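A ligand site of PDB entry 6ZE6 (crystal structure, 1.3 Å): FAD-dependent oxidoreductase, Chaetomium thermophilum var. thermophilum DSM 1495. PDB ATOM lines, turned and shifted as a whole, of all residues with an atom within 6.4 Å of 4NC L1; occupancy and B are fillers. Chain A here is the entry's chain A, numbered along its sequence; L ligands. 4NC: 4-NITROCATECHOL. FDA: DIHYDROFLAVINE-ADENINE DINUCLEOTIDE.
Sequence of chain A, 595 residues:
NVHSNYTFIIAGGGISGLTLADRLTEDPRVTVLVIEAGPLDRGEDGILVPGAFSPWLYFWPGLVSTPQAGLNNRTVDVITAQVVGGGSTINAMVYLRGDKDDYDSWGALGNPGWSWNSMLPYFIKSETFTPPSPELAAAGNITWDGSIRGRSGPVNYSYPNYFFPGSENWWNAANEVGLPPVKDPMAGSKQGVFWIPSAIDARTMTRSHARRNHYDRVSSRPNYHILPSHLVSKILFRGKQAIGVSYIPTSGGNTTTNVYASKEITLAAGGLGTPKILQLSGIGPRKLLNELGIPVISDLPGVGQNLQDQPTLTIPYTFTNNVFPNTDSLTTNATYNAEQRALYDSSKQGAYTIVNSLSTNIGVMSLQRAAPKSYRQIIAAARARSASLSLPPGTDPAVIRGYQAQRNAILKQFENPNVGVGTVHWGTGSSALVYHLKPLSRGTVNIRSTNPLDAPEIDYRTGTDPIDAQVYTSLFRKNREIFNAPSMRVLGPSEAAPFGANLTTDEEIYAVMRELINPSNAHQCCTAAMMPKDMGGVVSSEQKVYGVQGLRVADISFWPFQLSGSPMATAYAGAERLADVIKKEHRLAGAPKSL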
ATOM      1  N   VAL A  94      19.905 -32.557  14.048  1.00  0.00           N
ATOM      2  CA  VAL A  94      20.484 -31.510  13.173  1.00  0.00           C
ATOM      3  C   VAL A  94      20.687 -30.251  14.027  1.00  0.00           C
ATOM      4  O   VAL A  94      19.691 -29.699  14.545  1.00  0.00           O
ATOM      5  CB  VAL A  94      19.584 -31.259  11.980  1.00  0.00           C
ATOM      6  CG1 VAL A  94      20.054 -30.057  11.170  1.00  0.00           C
ATOM      7  CG2 VAL A  94      19.453 -32.519  11.113  1.00  0.00           C
ATOM      8  N   LEU A  96      22.053 -26.564  14.081  1.00  0.00           N
ATOM      9  CA  LEU A  96      22.403 -25.434  13.214  1.00  0.00           C
ATOM     10  C   LEU A  96      21.872 -24.157  13.825  1.00  0.00           C
ATOM     11  O   LEU A  96      20.704 -24.101  14.229  1.00  0.00           O
ATOM     12  CB  LEU A  96      21.783 -25.602  11.834  1.00  0.00           C
ATOM     13  CG  LEU A  96      22.501 -26.581  10.910  1.00  0.00           C
ATOM     14  CD1 LEU A  96      21.665 -26.805   9.688  1.00  0.00           C
ATOM     15  CD2 LEU A  96      23.877 -26.055  10.517  1.00  0.00           C
ATOM     16  N   ARG A  97      22.693 -23.122  13.875  1.00  0.00           N
ATOM     17  CA  ARG A  97      22.271 -21.767  14.235  1.00  0.00           C
ATOM     18  C   ARG A  97      21.523 -21.147  13.049  1.00  0.00           C
ATOM     19  O   ARG A  97      21.687 -21.565  11.896  1.00  0.00           O
ATOM     20  CB  ARG A  97      23.464 -20.883  14.558  1.00  0.00           C
ATOM     21  CG  ARG A  97      24.305 -21.414  15.692  1.00  0.00           C
ATOM     22  CD  ARG A  97      25.591 -20.645  15.879  1.00  0.00           C
ATOM     23  NE  ARG A  97      26.433 -21.293  16.853  1.00  0.00           N
ATOM     24  CZ  ARG A  97      27.687 -20.941  17.116  1.00  0.00           C
ATOM     25  NH1 ARG A  97      28.295 -20.004  16.393  1.00  0.00           N
ATOM     26  NH2 ARG A  97      28.359 -21.530  18.088  1.00  0.00           N
ATOM     27  N   LYS A 190      25.000 -19.324   5.616  1.00  0.00           N
ATOM     28  CA  LYS A 190      25.112 -20.746   5.200  1.00  0.00           C
ATOM     29  C   LYS A 190      24.686 -20.903   3.751  1.00  0.00           C
ATOM     30  O   LYS A 190      23.938 -21.847   3.418  1.00  0.00           O
ATOM     31  CB  LYS A 190      24.335 -21.603   6.173  1.00  0.00           C
ATOM     32  CG  LYS A 190      22.863 -21.310   6.299  1.00  0.00           C
ATOM     33  CD  LYS A 190      22.132 -22.232   7.299  1.00  0.00           C
ATOM     34  CE  LYS A 190      22.523 -22.001   8.739  1.00  0.00           C
ATOM     35  NZ  LYS A 190      21.980 -20.723   9.275  1.00  0.00           N
ATOM     36  N   PHE A 194      27.290 -27.903   3.036  1.00  0.00           N
ATOM     37  CA  PHE A 194      28.112 -28.120   4.216  1.00  0.00           C
ATOM     38  C   PHE A 194      27.705 -29.422   4.872  1.00  0.00           C
ATOM     39  O   PHE A 194      26.608 -29.947   4.698  1.00  0.00           O
ATOM     40  CB  PHE A 194      27.988 -26.963   5.203  1.00  0.00           C
ATOM     41  CG  PHE A 194      26.569 -26.548   5.461  1.00  0.00           C
ATOM     42  CD1 PHE A 194      25.928 -25.614   4.648  1.00  0.00           C
ATOM     43  CD2 PHE A 194      25.831 -27.130   6.496  1.00  0.00           C
ATOM     44  CE1 PHE A 194      24.612 -25.250   4.884  1.00  0.00           C
ATOM     45  CE2 PHE A 194      24.533 -26.738   6.735  1.00  0.00           C
ATOM     46  CZ  PHE A 194      23.914 -25.799   5.918  1.00  0.00           C
ATOM     47  N   GLN A 310       8.118 -25.282   9.529  1.00  0.00           N
ATOM     48  CA  GLN A 310       8.996 -25.253   8.325  1.00  0.00           C
ATOM     49  C   GLN A 310       8.610 -26.460   7.492  1.00  0.00           C
ATOM     50  O   GLN A 310       9.074 -27.588   7.735  1.00  0.00           O
ATOM     51  CB  GLN A 310      10.463 -25.207   8.682  1.00  0.00           C
ATOM     52  CG  GLN A 310      10.824 -23.937   9.414  1.00  0.00           C
ATOM     53  CD  GLN A 310      12.256 -23.811   9.833  1.00  0.00           C
ATOM     54  OE1 GLN A 310      12.777 -24.753  10.469  1.00  0.00           O
ATOM     55  NE2 GLN A 310      12.908 -22.697   9.527  1.00  0.00           N
ATOM     56  N   ILE A 362      24.225 -31.086   3.299  1.00  0.00           N
ATOM     57  CA  ILE A 362      22.944 -30.418   3.065  1.00  0.00           C
ATOM     58  C   ILE A 362      23.275 -29.114   2.344  1.00  0.00           C
ATOM     59  O   ILE A 362      24.400 -28.635   2.406  1.00  0.00           O
ATOM     60  CB  ILE A 362      22.164 -30.218   4.380  1.00  0.00           C
ATOM     61  CG1 ILE A 362      20.665 -30.000   4.177  1.00  0.00           C
ATOM     62  CG2 ILE A 362      22.822 -29.139   5.219  1.00  0.00           C
ATOM     63  CD1 ILE A 362      19.816 -30.348   5.356  1.00  0.00           C
ATOM     64  N   GLY A 363      22.243 -28.521   1.770  1.00  0.00           N
ATOM     65  CA  GLY A 363      22.348 -27.213   1.140  1.00  0.00           C
ATOM     66  C   GLY A 363      21.277 -26.252   1.598  1.00  0.00           C
ATOM     67  O   GLY A 363      20.144 -26.659   1.794  1.00  0.00           O
ATOM     68  N   VAL A 364      21.662 -24.982   1.703  1.00  0.00           N
ATOM     69  CA  VAL A 364      20.723 -23.908   2.062  1.00  0.00           C
ATOM     70  C   VAL A 364      20.903 -22.799   1.037  1.00  0.00           C
ATOM     71  O   VAL A 364      22.019 -22.530   0.605  1.00  0.00           O
ATOM     72  CB  VAL A 364      20.909 -23.430   3.516  1.00  0.00           C
ATOM     73  CG1 VAL A 364      20.039 -22.235   3.830  1.00  0.00           C
ATOM     74  CG2 VAL A 364      20.653 -24.557   4.486  1.00  0.00           C
ATOM     75  N   GLY A 422      15.309 -21.828   2.114  1.00  0.00           N
ATOM     76  CA  GLY A 422      14.977 -23.222   1.840  1.00  0.00           C
ATOM     77  C   GLY A 422      16.218 -24.085   1.905  1.00  0.00           C
ATOM     78  O   GLY A 422      17.339 -23.564   1.804  1.00  0.00           O
ATOM     79  N   THR A 423      15.960 -25.379   2.004  1.00  0.00           N
ATOM     80  CA  THR A 423      16.980 -26.433   2.201  1.00  0.00           C
ATOM     81  C   THR A 423      16.805 -27.476   1.086  1.00  0.00           C
ATOM     82  O   THR A 423      15.652 -27.753   0.745  1.00  0.00           O
ATOM     83  CB  THR A 423      16.903 -26.933   3.663  1.00  0.00           C
ATOM     84  OG1 THR A 423      17.065 -25.783   4.498  1.00  0.00           O
ATOM     85  CG2 THR A 423      17.969 -27.915   4.114  1.00  0.00           C
ATOM     86  N   TYR A 435      12.994 -28.376   2.117  1.00  0.00           N
ATOM     87  CA  TYR A 435      12.326 -27.703   3.243  1.00  0.00           C
ATOM     88  C   TYR A 435      12.131 -26.214   2.948  1.00  0.00           C
ATOM     89  O   TYR A 435      13.018 -25.596   2.368  1.00  0.00           O
ATOM     90  CB  TYR A 435      13.117 -27.819   4.552  1.00  0.00           C
ATOM     91  CG  TYR A 435      13.401 -29.219   5.021  1.00  0.00           C
ATOM     92  CD1 TYR A 435      12.660 -30.334   4.629  1.00  0.00           C
ATOM     93  CD2 TYR A 435      14.430 -29.444   5.888  1.00  0.00           C
ATOM     94  CE1 TYR A 435      12.898 -31.595   5.158  1.00  0.00           C
ATOM     95  CE2 TYR A 435      14.717 -30.705   6.400  1.00  0.00           C
ATOM     96  CZ  TYR A 435      13.932 -31.781   6.041  1.00  0.00           C
ATOM     97  OH  TYR A 435      14.173 -33.016   6.589  1.00  0.00           O
ATOM     98  N   LEU A 437      11.902 -22.799   4.710  1.00  0.00           N
ATOM     99  CA  LEU A 437      12.341 -22.294   6.023  1.00  0.00           C
ATOM    100  C   LEU A 437      11.581 -21.047   6.474  1.00  0.00           C
ATOM    101  O   LEU A 437      11.569 -20.786   7.676  1.00  0.00           O
ATOM    102  CB  LEU A 437      13.843 -22.007   6.032  1.00  0.00           C
ATOM    103  CG  LEU A 437      14.750 -23.162   5.685  1.00  0.00           C
ATOM    104  CD1 LEU A 437      16.177 -22.723   5.734  1.00  0.00           C
ATOM    105  CD2 LEU A 437      14.489 -24.337   6.592  1.00  0.00           C
ATOM    106  N   ASN A 521       7.788 -29.894  10.166  1.00  0.00           N
ATOM    107  CA  ASN A 521       8.957 -30.749  10.498  1.00  0.00           C
ATOM    108  C   ASN A 521       9.091 -30.794  12.029  1.00  0.00           C
ATOM    109  O   ASN A 521      10.211 -30.973  12.506  1.00  0.00           O
ATOM    110  CB  ASN A 521      10.224 -30.229   9.834  1.00  0.00           C
ATOM    111  CG  ASN A 521      11.284 -31.256   9.590  1.00  0.00           C
ATOM    112  OD1 ASN A 521      11.050 -32.451   9.839  1.00  0.00           O
ATOM    113  ND2 ASN A 521      12.425 -30.795   9.039  1.00  0.00           N
ATOM    114  N   HIS A 523       8.776 -28.253  13.982  1.00  0.00           N
ATOM    115  CA  HIS A 523       9.484 -27.013  14.326  1.00  0.00           C
ATOM    116  C   HIS A 523       8.475 -25.951  14.778  1.00  0.00           C
ATOM    117  O   HIS A 523       8.737 -24.755  14.588  1.00  0.00           O
ATOM    118  CB  HIS A 523      10.302 -26.502  13.156  1.00  0.00           C
ATOM    119  CG  HIS A 523      11.399 -27.406  12.708  1.00  0.00           C
ATOM    120  ND1 HIS A 523      12.213 -27.062  11.643  1.00  0.00           N
ATOM    121  CD2 HIS A 523      11.830 -28.613  13.123  1.00  0.00           C
ATOM    122  CE1 HIS A 523      13.081 -28.047  11.404  1.00  0.00           C
ATOM    123  NE2 HIS A 523      12.882 -29.005  12.305  1.00  0.00           N
ATOM    124  N   LEU A 563      13.673 -19.308  11.746  1.00  0.00           N
ATOM    125  CA  LEU A 563      15.091 -19.067  11.364  1.00  0.00           C
ATOM    126  C   LEU A 563      15.421 -19.598   9.975  1.00  0.00           C
ATOM    127  O   LEU A 563      14.800 -20.526   9.455  1.00  0.00           O
ATOM    128  CB  LEU A 563      15.993 -19.809  12.337  1.00  0.00           C
ATOM    129  CG  LEU A 563      15.800 -19.508  13.801  1.00  0.00           C
ATOM    130  CD1 LEU A 563      16.661 -20.492  14.621  1.00  0.00           C
ATOM    131  CD2 LEU A 563      16.127 -18.084  14.193  1.00  0.00           C
ATOM    132  N   SER A 564      16.536 -19.103   9.472  1.00  0.00           N
ATOM    133  CA  SER A 564      17.298 -19.782   8.403  1.00  0.00           C
ATOM    134  C   SER A 564      18.084 -20.892   9.095  1.00  0.00           C
ATOM    135  O   SER A 564      19.262 -20.728   9.391  1.00  0.00           O
ATOM    136  CB  SER A 564      18.181 -18.824   7.633  1.00  0.00           C
ATOM    137  OG  SER A 564      18.985 -19.523   6.705  1.00  0.00           O
ATOM    138  N   GLY A 565      17.403 -21.992   9.382  1.00  0.00           N
ATOM    139  CA  GLY A 565      17.989 -23.057  10.202  1.00  0.00           C
ATOM    140  C   GLY A 565      16.883 -23.845  10.838  1.00  0.00           C
ATOM    141  O   GLY A 565      15.757 -23.484  10.745  1.00  0.00           O
ATOM    142  N   SER A 566      17.228 -24.830  11.617  1.00  0.00           N
ATOM    143  CA  SER A 566      16.308 -25.617  12.430  1.00  0.00           C
ATOM    144  C   SER A 566      16.415 -25.138  13.884  1.00  0.00           C
ATOM    145  O   SER A 566      17.403 -24.520  14.260  1.00  0.00           O
ATOM    146  CB  SER A 566      16.587 -27.101  12.266  1.00  0.00           C
ATOM    147  OG  SER A 566      17.899 -27.381  12.692  1.00  0.00           O
ATOM    148  N   PRO A 567      15.386 -25.338  14.725  1.00  0.00           N
ATOM    149  CA  PRO A 567      15.346 -24.616  16.012  1.00  0.00           C
ATOM    150  C   PRO A 567      16.287 -25.028  17.142  1.00  0.00           C
ATOM    151  O   PRO A 567      16.529 -24.163  18.001  1.00  0.00           O
ATOM    152  CB  PRO A 567      13.898 -24.840  16.510  1.00  0.00           C
ATOM    153  CG  PRO A 567      13.140 -25.192  15.267  1.00  0.00           C
ATOM    154  CD  PRO A 567      14.112 -25.970  14.393  1.00  0.00           C
HETATM  155  C1  4NC L   1      16.225 -28.200   8.805  1.00  0.00           C
HETATM  156  C2  4NC L   1      16.055 -26.821   8.745  1.00  0.00           C
HETATM  157  C3  4NC L   1      17.107 -26.051   8.283  1.00  0.00           C
HETATM  158  C4  4NC L   1      18.298 -26.667   7.914  1.00  0.00           C
HETATM  159  C5  4NC L   1      18.458 -28.057   7.957  1.00  0.00           C
HETATM  160  C6  4NC L   1      17.420 -28.808   8.441  1.00  0.00           C
HETATM  161  O7  4NC L   1      15.166 -28.920   9.255  1.00  0.00           O
HETATM  162  O8  4NC L   1      14.830 -26.367   9.154  1.00  0.00           O
HETATM  163  N9  4NC L   1      19.401 -25.871   7.431  1.00  0.00           N
HETATM  164  O10 4NC L   1      20.336 -26.427   6.904  1.00  0.00           O
HETATM  165  O11 4NC L   1      19.344 -24.654   7.600  1.00  0.00           O
HETATM  166  PA  FDA L   2      10.258 -28.948  23.486  1.00  0.00           P
HETATM  167  O1A FDA L   2       9.253 -29.583  22.521  1.00  0.00           O
HETATM  168  O2A FDA L   2      11.694 -29.400  23.417  1.00  0.00           O
HETATM  169  O5B FDA L   2       9.761 -29.226  24.947  1.00  0.00           O
HETATM  170  C5B FDA L   2       8.452 -28.880  25.390  1.00  0.00           C
HETATM  171  C4B FDA L   2       8.094 -29.902  26.477  1.00  0.00           C
HETATM  172  O4B FDA L   2       6.879 -29.462  27.123  1.00  0.00           O
HETATM  173  C3B FDA L   2       7.812 -31.342  25.953  1.00  0.00           C
HETATM  174  O3B FDA L   2       8.738 -32.285  26.494  1.00  0.00           O
HETATM  175  C2B FDA L   2       6.350 -31.612  26.393  1.00  0.00           C
HETATM  176  O2B FDA L   2       6.086 -32.941  26.796  1.00  0.00           O
HETATM  177  C1B FDA L   2       6.161 -30.610  27.516  1.00  0.00           C
HETATM  178  N9A FDA L   2       4.805 -30.199  27.790  1.00  0.00           N
HETATM  179  C8A FDA L   2       3.890 -29.685  26.904  1.00  0.00           C
HETATM  180  N7A FDA L   2       2.780 -29.282  27.525  1.00  0.00           N
HETATM  181  C5A FDA L   2       3.025 -29.460  28.874  1.00  0.00           C
HETATM  182  C6A FDA L   2       2.276 -29.143  30.019  1.00  0.00           C
HETATM  183  N6A FDA L   2       1.070 -28.569  29.978  1.00  0.00           N
HETATM  184  N1A FDA L   2       2.814 -29.459  31.214  1.00  0.00           N
HETATM  185  C2A FDA L   2       3.997 -30.050  31.237  1.00  0.00           C
HETATM  186  N3A FDA L   2       4.800 -30.360  30.223  1.00  0.00           N
HETATM  187  C4A FDA L   2       4.259 -30.041  29.046  1.00  0.00           C
HETATM  188  N1  FDA L   2      15.086 -29.300  15.447  1.00  0.00           N
HETATM  189  C2  FDA L   2      16.367 -29.206  14.980  1.00  0.00           C
HETATM  190  O2  FDA L   2      17.010 -28.170  15.129  1.00  0.00           O
HETATM  191  N3  FDA L   2      16.960 -30.327  14.460  1.00  0.00           N
HETATM  192  C4  FDA L   2      16.291 -31.506  14.152  1.00  0.00           C
HETATM  193  O4  FDA L   2      16.888 -32.472  13.648  1.00  0.00           O
HETATM  194  C4X FDA L   2      14.919 -31.511  14.509  1.00  0.00           C
HETATM  195  N5  FDA L   2      14.131 -32.591  14.240  1.00  0.00           N
HETATM  196  C5X FDA L   2      12.925 -32.777  14.873  1.00  0.00           C
HETATM  197  C6  FDA L   2      12.281 -34.003  14.823  1.00  0.00           C
HETATM  198  C7  FDA L   2      11.248 -34.309  15.674  1.00  0.00           C
HETATM  199  C7M FDA L   2      10.587 -35.673  15.572  1.00  0.00           C
HETATM  200  C8  FDA L   2      10.842 -33.328  16.614  1.00  0.00           C
HETATM  201  C8M FDA L   2       9.723 -33.616  17.586  1.00  0.00           C
HETATM  202  C9  FDA L   2      11.443 -32.094  16.645  1.00  0.00           C
HETATM  203  C9A FDA L   2      12.475 -31.780  15.762  1.00  0.00           C
HETATM  204  N10 FDA L   2      13.162 -30.562  15.791  1.00  0.00           N
HETATM  205  C10 FDA L   2      14.385 -30.453  15.223  1.00  0.00           C
HETATM  206  C1' FDA L   2      12.559 -29.409  16.512  1.00  0.00           C
HETATM  207  C2' FDA L   2      13.170 -29.153  17.860  1.00  0.00           C
HETATM  208  O2' FDA L   2      13.530 -30.336  18.516  1.00  0.00           O
HETATM  209  C3' FDA L   2      12.161 -28.343  18.693  1.00  0.00           C
HETATM  210  O3' FDA L   2      11.867 -27.125  17.950  1.00  0.00           O
HETATM  211  C4' FDA L   2      12.672 -27.963  20.066  1.00  0.00           C
HETATM  212  O4' FDA L   2      12.790 -29.164  20.880  1.00  0.00           O
HETATM  213  C5' FDA L   2      11.790 -26.962  20.759  1.00  0.00           C
HETATM  214  O5' FDA L   2      12.266 -26.784  22.115  1.00  0.00           O
HETATM  215  P   FDA L   2      11.231 -26.226  23.204  1.00  0.00           P
HETATM  216  O1P FDA L   2      12.013 -26.124  24.479  1.00  0.00           O
HETATM  217  O2P FDA L   2      10.524 -25.065  22.633  1.00  0.00           O
HETATM  218  O3P FDA L   2      10.119 -27.401  23.258  1.00  0.00           O
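The side-chain amide oxygen (OE1) of Gln 310 lies within hydrogen-bond range of an oxygen (O8) of 4NC L1, at 2.9 Å.
ND2 of Asn 521 is in hydrogen-bond range of O7 of 4NC L1.
An oxygen (O8) of 4NC L1 sits at hydrogen-bond distance from the backbone carbonyl oxygen (O) of Gly 565.
An oxygen (O2) of FDA L2 is in hydrogen-bond range of the side-chain hydroxyl (OG) of Ser 566 (2.7 Å).
The backbone NH (N) of Val 94 sits at hydrogen-bond distance from an oxygen (O4) of FDA L2, at 3.0 Å.
N3 of FDA L2 lies within hydrogen-bond range of O of Val 94 (2.8 Å).
A ring nitrogen (ND1) of His 523 is in hydrogen-bond range of the side-chain amide oxygen (OE1) of Gln 310, at 2.7 Å.
O of Leu 437 sits at hydrogen-bond distance from NE2 of Gln 310.
The backbone carbonyl oxygen (O) of Gly 565 sits at hydrogen-bond distance from the side-chain amide nitrogen (NE2) of Gln 310 (3.2 Å).
The side-chain amide nitrogen of Gln 310 sits at hydrogen-bond distance from the backbone carbonyl oxygen of Leu 563 (2.9 Å).
A ring nitrogen (NE2) of His 523 lies close to the backbone carbonyl oxygen (O) of Asn 521, at 3.3 Å.
OG of Ser 566 is in hydrogen-bond range of O of Val 94.
The side-chain amino group (NZ) of Lys 190 sits at hydrogen-bond distance from the backbone carbonyl oxygen (O) of Ser 564 (2.7 Å).
O of Phe 194 sits at hydrogen-bond distance from N of Ile 362.
Val 94 touches 4NC L1 (CG1 to C6, 3.99 Å).
Leu 96 touches 4NC L1.
Lys 190 touches 4NC L1 (CD to O11, 3.7 Å).
Phe 194 touches 4NC L1.
Ile 362 touches 4NC L1 (CD1 to C5, 3.7 Å).
Val 364 touches 4NC L1 (CG2 to O10, 3.1 Å).
Thr 423 touches 4NC L1 (OG1 to C4, 3.7 Å).
CE2 of Tyr 435 touches O7 of 4NC L1, 3.4 Å away.
Leu 437 touches 4NC L1 (CD2 to O8, 3.3 Å).
His 523 touches 4NC L1.
Ser 566 touches 4NC L1 (N to C3, 3.6 Å).
Hydrophobic or aromatic side chains that line 4NC L1: Val 94, Leu 96, Phe 194, Ile 362, Val 364, Tyr 435, Leu 437 and His 523.
Of the 20 residues printed, 14 come within 4 Å of 4NC L1.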
